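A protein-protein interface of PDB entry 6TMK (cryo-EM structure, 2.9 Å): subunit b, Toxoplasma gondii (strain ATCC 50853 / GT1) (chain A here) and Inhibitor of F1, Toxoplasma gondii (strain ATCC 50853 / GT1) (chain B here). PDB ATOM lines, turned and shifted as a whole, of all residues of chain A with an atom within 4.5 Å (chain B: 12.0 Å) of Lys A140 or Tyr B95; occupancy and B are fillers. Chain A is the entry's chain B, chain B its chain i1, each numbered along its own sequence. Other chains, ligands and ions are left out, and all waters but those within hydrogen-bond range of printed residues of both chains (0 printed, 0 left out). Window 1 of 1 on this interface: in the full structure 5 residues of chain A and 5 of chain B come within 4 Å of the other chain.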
ATOM      1  N   LEU A 136     -18.100  21.362  -7.973  1.00  0.00           N
ATOM      2  CA  LEU A 136     -16.966  20.573  -7.508  1.00  0.00           C
ATOM      3  C   LEU A 136     -17.004  20.369  -6.003  1.00  0.00           C
ATOM      4  O   LEU A 136     -16.561  19.328  -5.513  1.00  0.00           O
ATOM      5  CB  LEU A 136     -15.663  21.248  -7.914  1.00  0.00           C
ATOM      6  CG  LEU A 136     -15.253  21.105  -9.376  1.00  0.00           C
ATOM      7  CD1 LEU A 136     -13.991  21.878  -9.633  1.00  0.00           C
ATOM      8  CD2 LEU A 136     -15.060  19.657  -9.751  1.00  0.00           C
ATOM      9  N   ARG A 137     -17.522  21.341  -5.256  1.00  0.00           N
ATOM     10  CA  ARG A 137     -17.692  21.151  -3.819  1.00  0.00           C
ATOM     11  C   ARG A 137     -18.622  19.975  -3.530  1.00  0.00           C
ATOM     12  O   ARG A 137     -18.273  19.046  -2.783  1.00  0.00           O
ATOM     13  CB  ARG A 137     -18.230  22.439  -3.204  1.00  0.00           C
ATOM     14  CG  ARG A 137     -17.729  22.721  -1.811  1.00  0.00           C
ATOM     15  CD  ARG A 137     -18.068  24.136  -1.384  1.00  0.00           C
ATOM     16  NE  ARG A 137     -17.300  25.130  -2.134  1.00  0.00           N
ATOM     17  CZ  ARG A 137     -17.814  26.047  -2.950  1.00  0.00           C
ATOM     18  NH1 ARG A 137     -19.122  26.133  -3.156  1.00  0.00           N
ATOM     19  NH2 ARG A 137     -17.008  26.891  -3.573  1.00  0.00           N
ATOM     20  N   PHE A 138     -19.821  20.012  -4.110  1.00  0.00           N
ATOM     21  CA  PHE A 138     -20.776  18.923  -3.950  1.00  0.00           C
ATOM     22  C   PHE A 138     -20.187  17.602  -4.426  1.00  0.00           C
ATOM     23  O   PHE A 138     -20.431  16.551  -3.822  1.00  0.00           O
ATOM     24  CB  PHE A 138     -22.051  19.255  -4.721  1.00  0.00           C
ATOM     25  CG  PHE A 138     -23.213  18.383  -4.375  1.00  0.00           C
ATOM     26  CD1 PHE A 138     -23.955  18.619  -3.238  1.00  0.00           C
ATOM     27  CD2 PHE A 138     -23.569  17.330  -5.192  1.00  0.00           C
ATOM     28  CE1 PHE A 138     -25.023  17.819  -2.919  1.00  0.00           C
ATOM     29  CE2 PHE A 138     -24.635  16.529  -4.876  1.00  0.00           C
ATOM     30  CZ  PHE A 138     -25.364  16.774  -3.738  1.00  0.00           C
ATOM     31  N   LEU A 139     -19.408  17.634  -5.505  1.00  0.00           N
ATOM     32  CA  LEU A 139     -18.812  16.408  -6.018  1.00  0.00           C
ATOM     33  C   LEU A 139     -17.794  15.845  -5.041  1.00  0.00           C
ATOM     34  O   LEU A 139     -17.720  14.628  -4.849  1.00  0.00           O
ATOM     35  CB  LEU A 139     -18.156  16.665  -7.369  1.00  0.00           C
ATOM     36  CG  LEU A 139     -17.514  15.436  -8.005  1.00  0.00           C
ATOM     37  CD1 LEU A 139     -18.576  14.480  -8.475  1.00  0.00           C
ATOM     38  CD2 LEU A 139     -16.607  15.832  -9.138  1.00  0.00           C
ATOM     39  N   LYS A 140     -16.981  16.708  -4.440  1.00  0.00           N
ATOM     40  CA  LYS A 140     -16.028  16.254  -3.440  1.00  0.00           C
ATOM     41  C   LYS A 140     -16.748  15.592  -2.280  1.00  0.00           C
ATOM     42  O   LYS A 140     -16.343  14.525  -1.807  1.00  0.00           O
ATOM     43  CB  LYS A 140     -15.196  17.429  -2.942  1.00  0.00           C
ATOM     44  CG  LYS A 140     -13.950  17.018  -2.199  1.00  0.00           C
ATOM     45  CD  LYS A 140     -13.329  18.192  -1.484  1.00  0.00           C
ATOM     46  CE  LYS A 140     -12.283  17.732  -0.494  1.00  0.00           C
ATOM     47  NZ  LYS A 140     -11.476  16.601  -1.021  1.00  0.00           N
ATOM     48  N   LEU A 141     -17.819  16.219  -1.805  1.00  0.00           N
ATOM     49  CA  LEU A 141     -18.614  15.613  -0.740  1.00  0.00           C
ATOM     50  C   LEU A 141     -19.132  14.234  -1.147  1.00  0.00           C
ATOM     51  O   LEU A 141     -18.970  13.245  -0.415  1.00  0.00           O
ATOM     52  CB  LEU A 141     -19.770  16.544  -0.387  1.00  0.00           C
ATOM     53  CG  LEU A 141     -20.842  16.009   0.547  1.00  0.00           C
ATOM     54  CD1 LEU A 141     -20.214  15.430   1.797  1.00  0.00           C
ATOM     55  CD2 LEU A 141     -21.795  17.131   0.885  1.00  0.00           C
ATOM     56  N   VAL A 142     -19.760  14.152  -2.321  1.00  0.00           N
ATOM     57  CA  VAL A 142     -20.359  12.899  -2.765  1.00  0.00           C
ATOM     58  C   VAL A 142     -19.301  11.817  -2.912  1.00  0.00           C
ATOM     59  O   VAL A 142     -19.531  10.654  -2.560  1.00  0.00           O
ATOM     60  CB  VAL A 142     -21.125  13.121  -4.081  1.00  0.00           C
ATOM     61  CG1 VAL A 142     -21.446  11.805  -4.738  1.00  0.00           C
ATOM     62  CG2 VAL A 142     -22.385  13.901  -3.823  1.00  0.00           C
ATOM     63  N   THR A 143     -18.134  12.171  -3.450  1.00  0.00           N
ATOM     64  CA  THR A 143     -17.081  11.183  -3.647  1.00  0.00           C
ATOM     65  C   THR A 143     -16.456  10.764  -2.326  1.00  0.00           C
ATOM     66  O   THR A 143     -16.053   9.607  -2.174  1.00  0.00           O
ATOM     67  CB  THR A 143     -16.012  11.735  -4.582  1.00  0.00           C
ATOM     68  OG1 THR A 143     -15.636  13.052  -4.162  1.00  0.00           O
ATOM     69  CG2 THR A 143     -16.536  11.788  -5.998  1.00  0.00           C
ATOM     70  N   ASP A 144     -16.367  11.681  -1.364  1.00  0.00           N
ATOM     71  CA  ASP A 144     -15.863  11.314  -0.049  1.00  0.00           C
ATOM     72  C   ASP A 144     -16.805  10.343   0.637  1.00  0.00           C
ATOM     73  O   ASP A 144     -16.361   9.483   1.406  1.00  0.00           O
ATOM     74  CB  ASP A 144     -15.669  12.560   0.813  1.00  0.00           C
ATOM     75  CG  ASP A 144     -14.468  13.382   0.389  1.00  0.00           C
ATOM     76  OD1 ASP A 144     -14.556  14.627   0.429  1.00  0.00           O
ATOM     77  OD2 ASP A 144     -13.437  12.785   0.015  1.00  0.00           O
ATOM     78  N   PHE A 152     -12.929  12.172  -8.657  1.00  0.00           N
ATOM     79  CA  PHE A 152     -12.986  13.597  -8.368  1.00  0.00           C
ATOM     80  C   PHE A 152     -11.714  14.285  -8.829  1.00  0.00           C
ATOM     81  O   PHE A 152     -11.763  15.362  -9.430  1.00  0.00           O
ATOM     82  CB  PHE A 152     -13.196  13.825  -6.877  1.00  0.00           C
ATOM     83  CG  PHE A 152     -12.986  15.243  -6.450  1.00  0.00           C
ATOM     84  CD1 PHE A 152     -13.956  16.197  -6.677  1.00  0.00           C
ATOM     85  CD2 PHE A 152     -11.817  15.627  -5.831  1.00  0.00           C
ATOM     86  CE1 PHE A 152     -13.764  17.502  -6.288  1.00  0.00           C
ATOM     87  CE2 PHE A 152     -11.623  16.931  -5.441  1.00  0.00           C
ATOM     88  CZ  PHE A 152     -12.596  17.868  -5.673  1.00  0.00           C
ATOM     89  N   ARG B  82       3.191  28.107  -6.016  1.00  0.00           N
ATOM     90  CA  ARG B  82       2.410  28.436  -7.201  1.00  0.00           C
ATOM     91  C   ARG B  82       1.706  27.201  -7.748  1.00  0.00           C
ATOM     92  O   ARG B  82       0.495  27.218  -7.991  1.00  0.00           O
ATOM     93  CB  ARG B  82       3.316  29.048  -8.269  1.00  0.00           C
ATOM     94  CG  ARG B  82       3.111  30.535  -8.488  1.00  0.00           C
ATOM     95  CD  ARG B  82       3.421  30.912  -9.921  1.00  0.00           C
ATOM     96  NE  ARG B  82       4.745  30.449 -10.325  1.00  0.00           N
ATOM     97  CZ  ARG B  82       5.876  31.098 -10.062  1.00  0.00           C
ATOM     98  NH1 ARG B  82       5.852  32.240  -9.388  1.00  0.00           N
ATOM     99  NH2 ARG B  82       7.034  30.599 -10.467  1.00  0.00           N
ATOM    100  N   ASN B  83       2.452  26.117  -7.949  1.00  0.00           N
ATOM    101  CA  ASN B  83       1.951  24.971  -8.699  1.00  0.00           C
ATOM    102  C   ASN B  83       1.383  23.858  -7.819  1.00  0.00           C
ATOM    103  O   ASN B  83       1.150  22.753  -8.317  1.00  0.00           O
ATOM    104  CB  ASN B  83       3.062  24.407  -9.586  1.00  0.00           C
ATOM    105  CG  ASN B  83       3.394  25.317 -10.750  1.00  0.00           C
ATOM    106  OD1 ASN B  83       2.574  26.136 -11.167  1.00  0.00           O
ATOM    107  ND2 ASN B  83       4.602  25.181 -11.281  1.00  0.00           N
ATOM    108  N   LEU B  84       1.152  24.117  -6.531  1.00  0.00           N
ATOM    109  CA  LEU B  84       0.641  23.072  -5.646  1.00  0.00           C
ATOM    110  C   LEU B  84      -0.839  22.796  -5.896  1.00  0.00           C
ATOM    111  O   LEU B  84      -1.220  21.679  -6.268  1.00  0.00           O
ATOM    112  CB  LEU B  84       0.866  23.468  -4.188  1.00  0.00           C
ATOM    113  CG  LEU B  84       0.575  22.368  -3.170  1.00  0.00           C
ATOM    114  CD1 LEU B  84       1.766  21.443  -3.033  1.00  0.00           C
ATOM    115  CD2 LEU B  84       0.212  22.964  -1.827  1.00  0.00           C
ATOM    116  N   LEU B  85      -1.682  23.814  -5.715  1.00  0.00           N
ATOM    117  CA  LEU B  85      -3.116  23.580  -5.576  1.00  0.00           C
ATOM    118  C   LEU B  85      -3.710  22.979  -6.840  1.00  0.00           C
ATOM    119  O   LEU B  85      -4.730  22.284  -6.777  1.00  0.00           O
ATOM    120  CB  LEU B  85      -3.829  24.882  -5.221  1.00  0.00           C
ATOM    121  CG  LEU B  85      -3.435  25.480  -3.872  1.00  0.00           C
ATOM    122  CD1 LEU B  85      -4.015  26.875  -3.714  1.00  0.00           C
ATOM    123  CD2 LEU B  85      -3.872  24.578  -2.737  1.00  0.00           C
ATOM    124  N   ALA B  86      -3.093  23.234  -7.992  1.00  0.00           N
ATOM    125  CA  ALA B  86      -3.543  22.603  -9.224  1.00  0.00           C
ATOM    126  C   ALA B  86      -3.364  21.094  -9.140  1.00  0.00           C
ATOM    127  O   ALA B  86      -4.325  20.329  -9.281  1.00  0.00           O
ATOM    128  CB  ALA B  86      -2.776  23.177 -10.415  1.00  0.00           C
ATOM    129  N   ASN B  87      -2.132  20.645  -8.909  1.00  0.00           N
ATOM    130  CA  ASN B  87      -1.826  19.224  -8.929  1.00  0.00           C
ATOM    131  C   ASN B  87      -2.296  18.498  -7.676  1.00  0.00           C
ATOM    132  O   ASN B  87      -2.224  17.266  -7.634  1.00  0.00           O
ATOM    133  CB  ASN B  87      -0.320  19.022  -9.096  1.00  0.00           C
ATOM    134  CG  ASN B  87       0.242  19.787 -10.275  1.00  0.00           C
ATOM    135  OD1 ASN B  87       0.143  19.348 -11.421  1.00  0.00           O
ATOM    136  ND2 ASN B  87       0.830  20.944 -10.001  1.00  0.00           N
ATOM    137  N   HIS B  88      -2.772  19.220  -6.663  1.00  0.00           N
ATOM    138  CA  HIS B  88      -3.272  18.607  -5.429  1.00  0.00           C
ATOM    139  C   HIS B  88      -4.530  19.337  -4.981  1.00  0.00           C
ATOM    140  O   HIS B  88      -4.541  20.033  -3.960  1.00  0.00           O
ATOM    141  CB  HIS B  88      -2.200  18.628  -4.339  1.00  0.00           C
ATOM    142  CG  HIS B  88      -0.892  18.044  -4.768  1.00  0.00           C
ATOM    143  ND1 HIS B  88       0.022  18.742  -5.527  1.00  0.00           N
ATOM    144  CD2 HIS B  88      -0.346  16.825  -4.549  1.00  0.00           C
ATOM    145  CE1 HIS B  88       1.075  17.980  -5.756  1.00  0.00           C
ATOM    146  NE2 HIS B  88       0.878  16.811  -5.172  1.00  0.00           N
ATOM    147  N   PRO B  89      -5.624  19.192  -5.733  1.00  0.00           N
ATOM    148  CA  PRO B  89      -6.849  19.932  -5.399  1.00  0.00           C
ATOM    149  C   PRO B  89      -7.578  19.396  -4.182  1.00  0.00           C
ATOM    150  O   PRO B  89      -8.424  20.108  -3.627  1.00  0.00           O
ATOM    151  CB  PRO B  89      -7.699  19.779  -6.663  1.00  0.00           C
ATOM    152  CG  PRO B  89      -7.266  18.485  -7.234  1.00  0.00           C
ATOM    153  CD  PRO B  89      -5.802  18.347  -6.925  1.00  0.00           C
ATOM    154  N   GLU B  90      -7.289  18.167  -3.753  1.00  0.00           N
ATOM    155  CA  GLU B  90      -7.946  17.613  -2.576  1.00  0.00           C
ATOM    156  C   GLU B  90      -7.664  18.424  -1.321  1.00  0.00           C
ATOM    157  O   GLU B  90      -8.444  18.361  -0.366  1.00  0.00           O
ATOM    158  CB  GLU B  90      -7.491  16.172  -2.349  1.00  0.00           C
ATOM    159  CG  GLU B  90      -5.979  15.997  -2.327  1.00  0.00           C
ATOM    160  CD  GLU B  90      -5.431  15.348  -3.578  1.00  0.00           C
ATOM    161  OE1 GLU B  90      -6.002  15.571  -4.662  1.00  0.00           O
ATOM    162  OE2 GLU B  90      -4.429  14.610  -3.478  1.00  0.00           O
ATOM    163  N   TYR B  91      -6.570  19.183  -1.303  1.00  0.00           N
ATOM    164  CA  TYR B  91      -6.292  20.112  -0.217  1.00  0.00           C
ATOM    165  C   TYR B  91      -6.911  21.484  -0.436  1.00  0.00           C
ATOM    166  O   TYR B  91      -7.201  22.185   0.540  1.00  0.00           O
ATOM    167  CB  TYR B  91      -4.779  20.263  -0.042  1.00  0.00           C
ATOM    168  CG  TYR B  91      -4.036  18.950  -0.063  1.00  0.00           C
ATOM    169  CD1 TYR B  91      -4.560  17.823   0.551  1.00  0.00           C
ATOM    170  CD2 TYR B  91      -2.812  18.835  -0.705  1.00  0.00           C
ATOM    171  CE1 TYR B  91      -3.888  16.621   0.529  1.00  0.00           C
ATOM    172  CE2 TYR B  91      -2.131  17.636  -0.733  1.00  0.00           C
ATOM    173  CZ  TYR B  91      -2.673  16.531  -0.114  1.00  0.00           C
ATOM    174  OH  TYR B  91      -2.001  15.333  -0.136  1.00  0.00           O
ATOM    175  N   ASP B  92      -7.121  21.880  -1.682  1.00  0.00           N
ATOM    176  CA  ASP B  92      -7.621  23.212  -1.983  1.00  0.00           C
ATOM    177  C   ASP B  92      -8.973  23.443  -1.317  1.00  0.00           C
ATOM    178  O   ASP B  92      -9.947  22.754  -1.658  1.00  0.00           O
ATOM    179  CB  ASP B  92      -7.748  23.398  -3.491  1.00  0.00           C
ATOM    180  CG  ASP B  92      -8.019  24.836  -3.881  1.00  0.00           C
ATOM    181  OD1 ASP B  92      -8.056  25.700  -2.982  1.00  0.00           O
ATOM    182  OD2 ASP B  92      -8.195  25.101  -5.088  1.00  0.00           O
ATOM    183  N   PRO B  93      -9.085  24.385  -0.373  1.00  0.00           N
ATOM    184  CA  PRO B  93     -10.389  24.642   0.253  1.00  0.00           C
ATOM    185  C   PRO B  93     -11.381  25.318  -0.672  1.00  0.00           C
ATOM    186  O   PRO B  93     -12.543  25.494  -0.284  1.00  0.00           O
ATOM    187  CB  PRO B  93     -10.031  25.555   1.434  1.00  0.00           C
ATOM    188  CG  PRO B  93      -8.597  25.267   1.697  1.00  0.00           C
ATOM    189  CD  PRO B  93      -8.019  25.111   0.330  1.00  0.00           C
ATOM    190  N   LYS B  94     -10.963  25.699  -1.880  1.00  0.00           N
ATOM    191  CA  LYS B  94     -11.912  26.212  -2.857  1.00  0.00           C
ATOM    192  C   LYS B  94     -12.966  25.169  -3.191  1.00  0.00           C
ATOM    193  O   LYS B  94     -14.120  25.513  -3.466  1.00  0.00           O
ATOM    194  CB  LYS B  94     -11.174  26.641  -4.123  1.00  0.00           C
ATOM    195  CG  LYS B  94     -12.025  27.413  -5.111  1.00  0.00           C
ATOM    196  CD  LYS B  94     -11.258  27.684  -6.394  1.00  0.00           C
ATOM    197  CE  LYS B  94     -12.112  28.431  -7.403  1.00  0.00           C
ATOM    198  NZ  LYS B  94     -11.324  28.880  -8.582  1.00  0.00           N
ATOM    199  N   TYR B  95     -12.587  23.891  -3.165  1.00  0.00           N
ATOM    200  CA  TYR B  95     -13.495  22.783  -3.424  1.00  0.00           C
ATOM    201  C   TYR B  95     -13.974  22.117  -2.140  1.00  0.00           C
ATOM    202  O   TYR B  95     -14.208  20.905  -2.119  1.00  0.00           O
ATOM    203  CB  TYR B  95     -12.825  21.755  -4.333  1.00  0.00           C
ATOM    204  CG  TYR B  95     -12.169  22.351  -5.554  1.00  0.00           C
ATOM    205  CD1 TYR B  95     -10.976  21.843  -6.042  1.00  0.00           C
ATOM    206  CD2 TYR B  95     -12.753  23.412  -6.229  1.00  0.00           C
ATOM    207  CE1 TYR B  95     -10.378  22.382  -7.161  1.00  0.00           C
ATOM    208  CE2 TYR B  95     -12.162  23.956  -7.347  1.00  0.00           C
ATOM    209  CZ  TYR B  95     -10.974  23.440  -7.809  1.00  0.00           C
ATOM    210  OH  TYR B  95     -10.385  23.982  -8.927  1.00  0.00           O
ATOM    211  N   SER B  96     -14.115  22.883  -1.065  1.00  0.00           N
ATOM    212  CA  SER B  96     -14.565  22.333   0.207  1.00  0.00           C
ATOM    213  C   SER B  96     -15.372  23.361   0.989  1.00  0.00           C
ATOM    214  O   SER B  96     -16.056  23.022   1.955  1.00  0.00           O
ATOM    215  CB  SER B  96     -13.378  21.860   1.042  1.00  0.00           C
ATOM    216  OG  SER B  96     -13.820  21.217   2.223  1.00  0.00           O
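Among the printed residues, pairs that only touch across the chains: Lys A140 with Tyr B95, Lys A140 with Glu B90, Leu A136 with Tyr B95, Arg A137 with Ser B96 and Arg A137 with Tyr B95.
Lys A140 touches two residues of chain B.
Tyr B95 touches just these residues of chain A: Leu A136 (3.6 Å), Arg A137 (3.8 Å) and Lys A140 (2.9 Å).
Leu A136 touches just one residue of chain B: Tyr B95 (3.6 Å).
Of the printed residues of chain B, Arg A137 touches Lys B94, Tyr B95 and Ser B96.
Leu A141 touches none of the printed residues of chain B.
No residue of chain B comes within 4 Å of Val A142.
No residue of chain B comes within 4 Å of Thr A143.
No residue of chain B comes within 4 Å of Asp A144.
Printed residues of chain A within 4 Å of Glu B90: Lys A140.
Of the printed residues of chain A, Lys B94 touches Arg A137 (3.2 Å).
Printed residues of chain A within 4 Å of Ser B96: Arg A137.
The nearest residue of chain B that does not touch Lys A140 is Ser B96 (4.5 Å).
Printed residues of chain A that touch a printed residue of chain B: Leu A136, Arg A137 and Lys A140.
Hydrophobic or aromatic side chains of chain A that line the printed part of chain B: Leu A136.
Of the 15 printed residues of chain B, 4 touch a printed residue of chain A.
Hydrophobic or aromatic side chains of chain B within 4 Å of the printed part of chain A: Tyr B95.
Among the printed residues, no Asp or Glu carboxylate lies within 4 Å of a Lys or Arg side-chain nitrogen of the other chain.
The side-chain hydroxyl (OG1) of Thr A143 lies within hydrogen-bond range of the backbone carbonyl oxygen (O) of Lys A140 (2.9 Å).
NZ of Lys A140 lies within salt-bridge range of OD1 of Asp A144 (3.9 Å).
The backbone NH (N) of Lys B94 sits close to the side-chain carboxylate (OD1) of Asp B92, at 3.1 Å.
The backbone carbonyl oxygen (O) of Lys B94 lies within hydrogen-bond range of the guanidinium group (NH2) of Arg A137 (3.2 Å).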
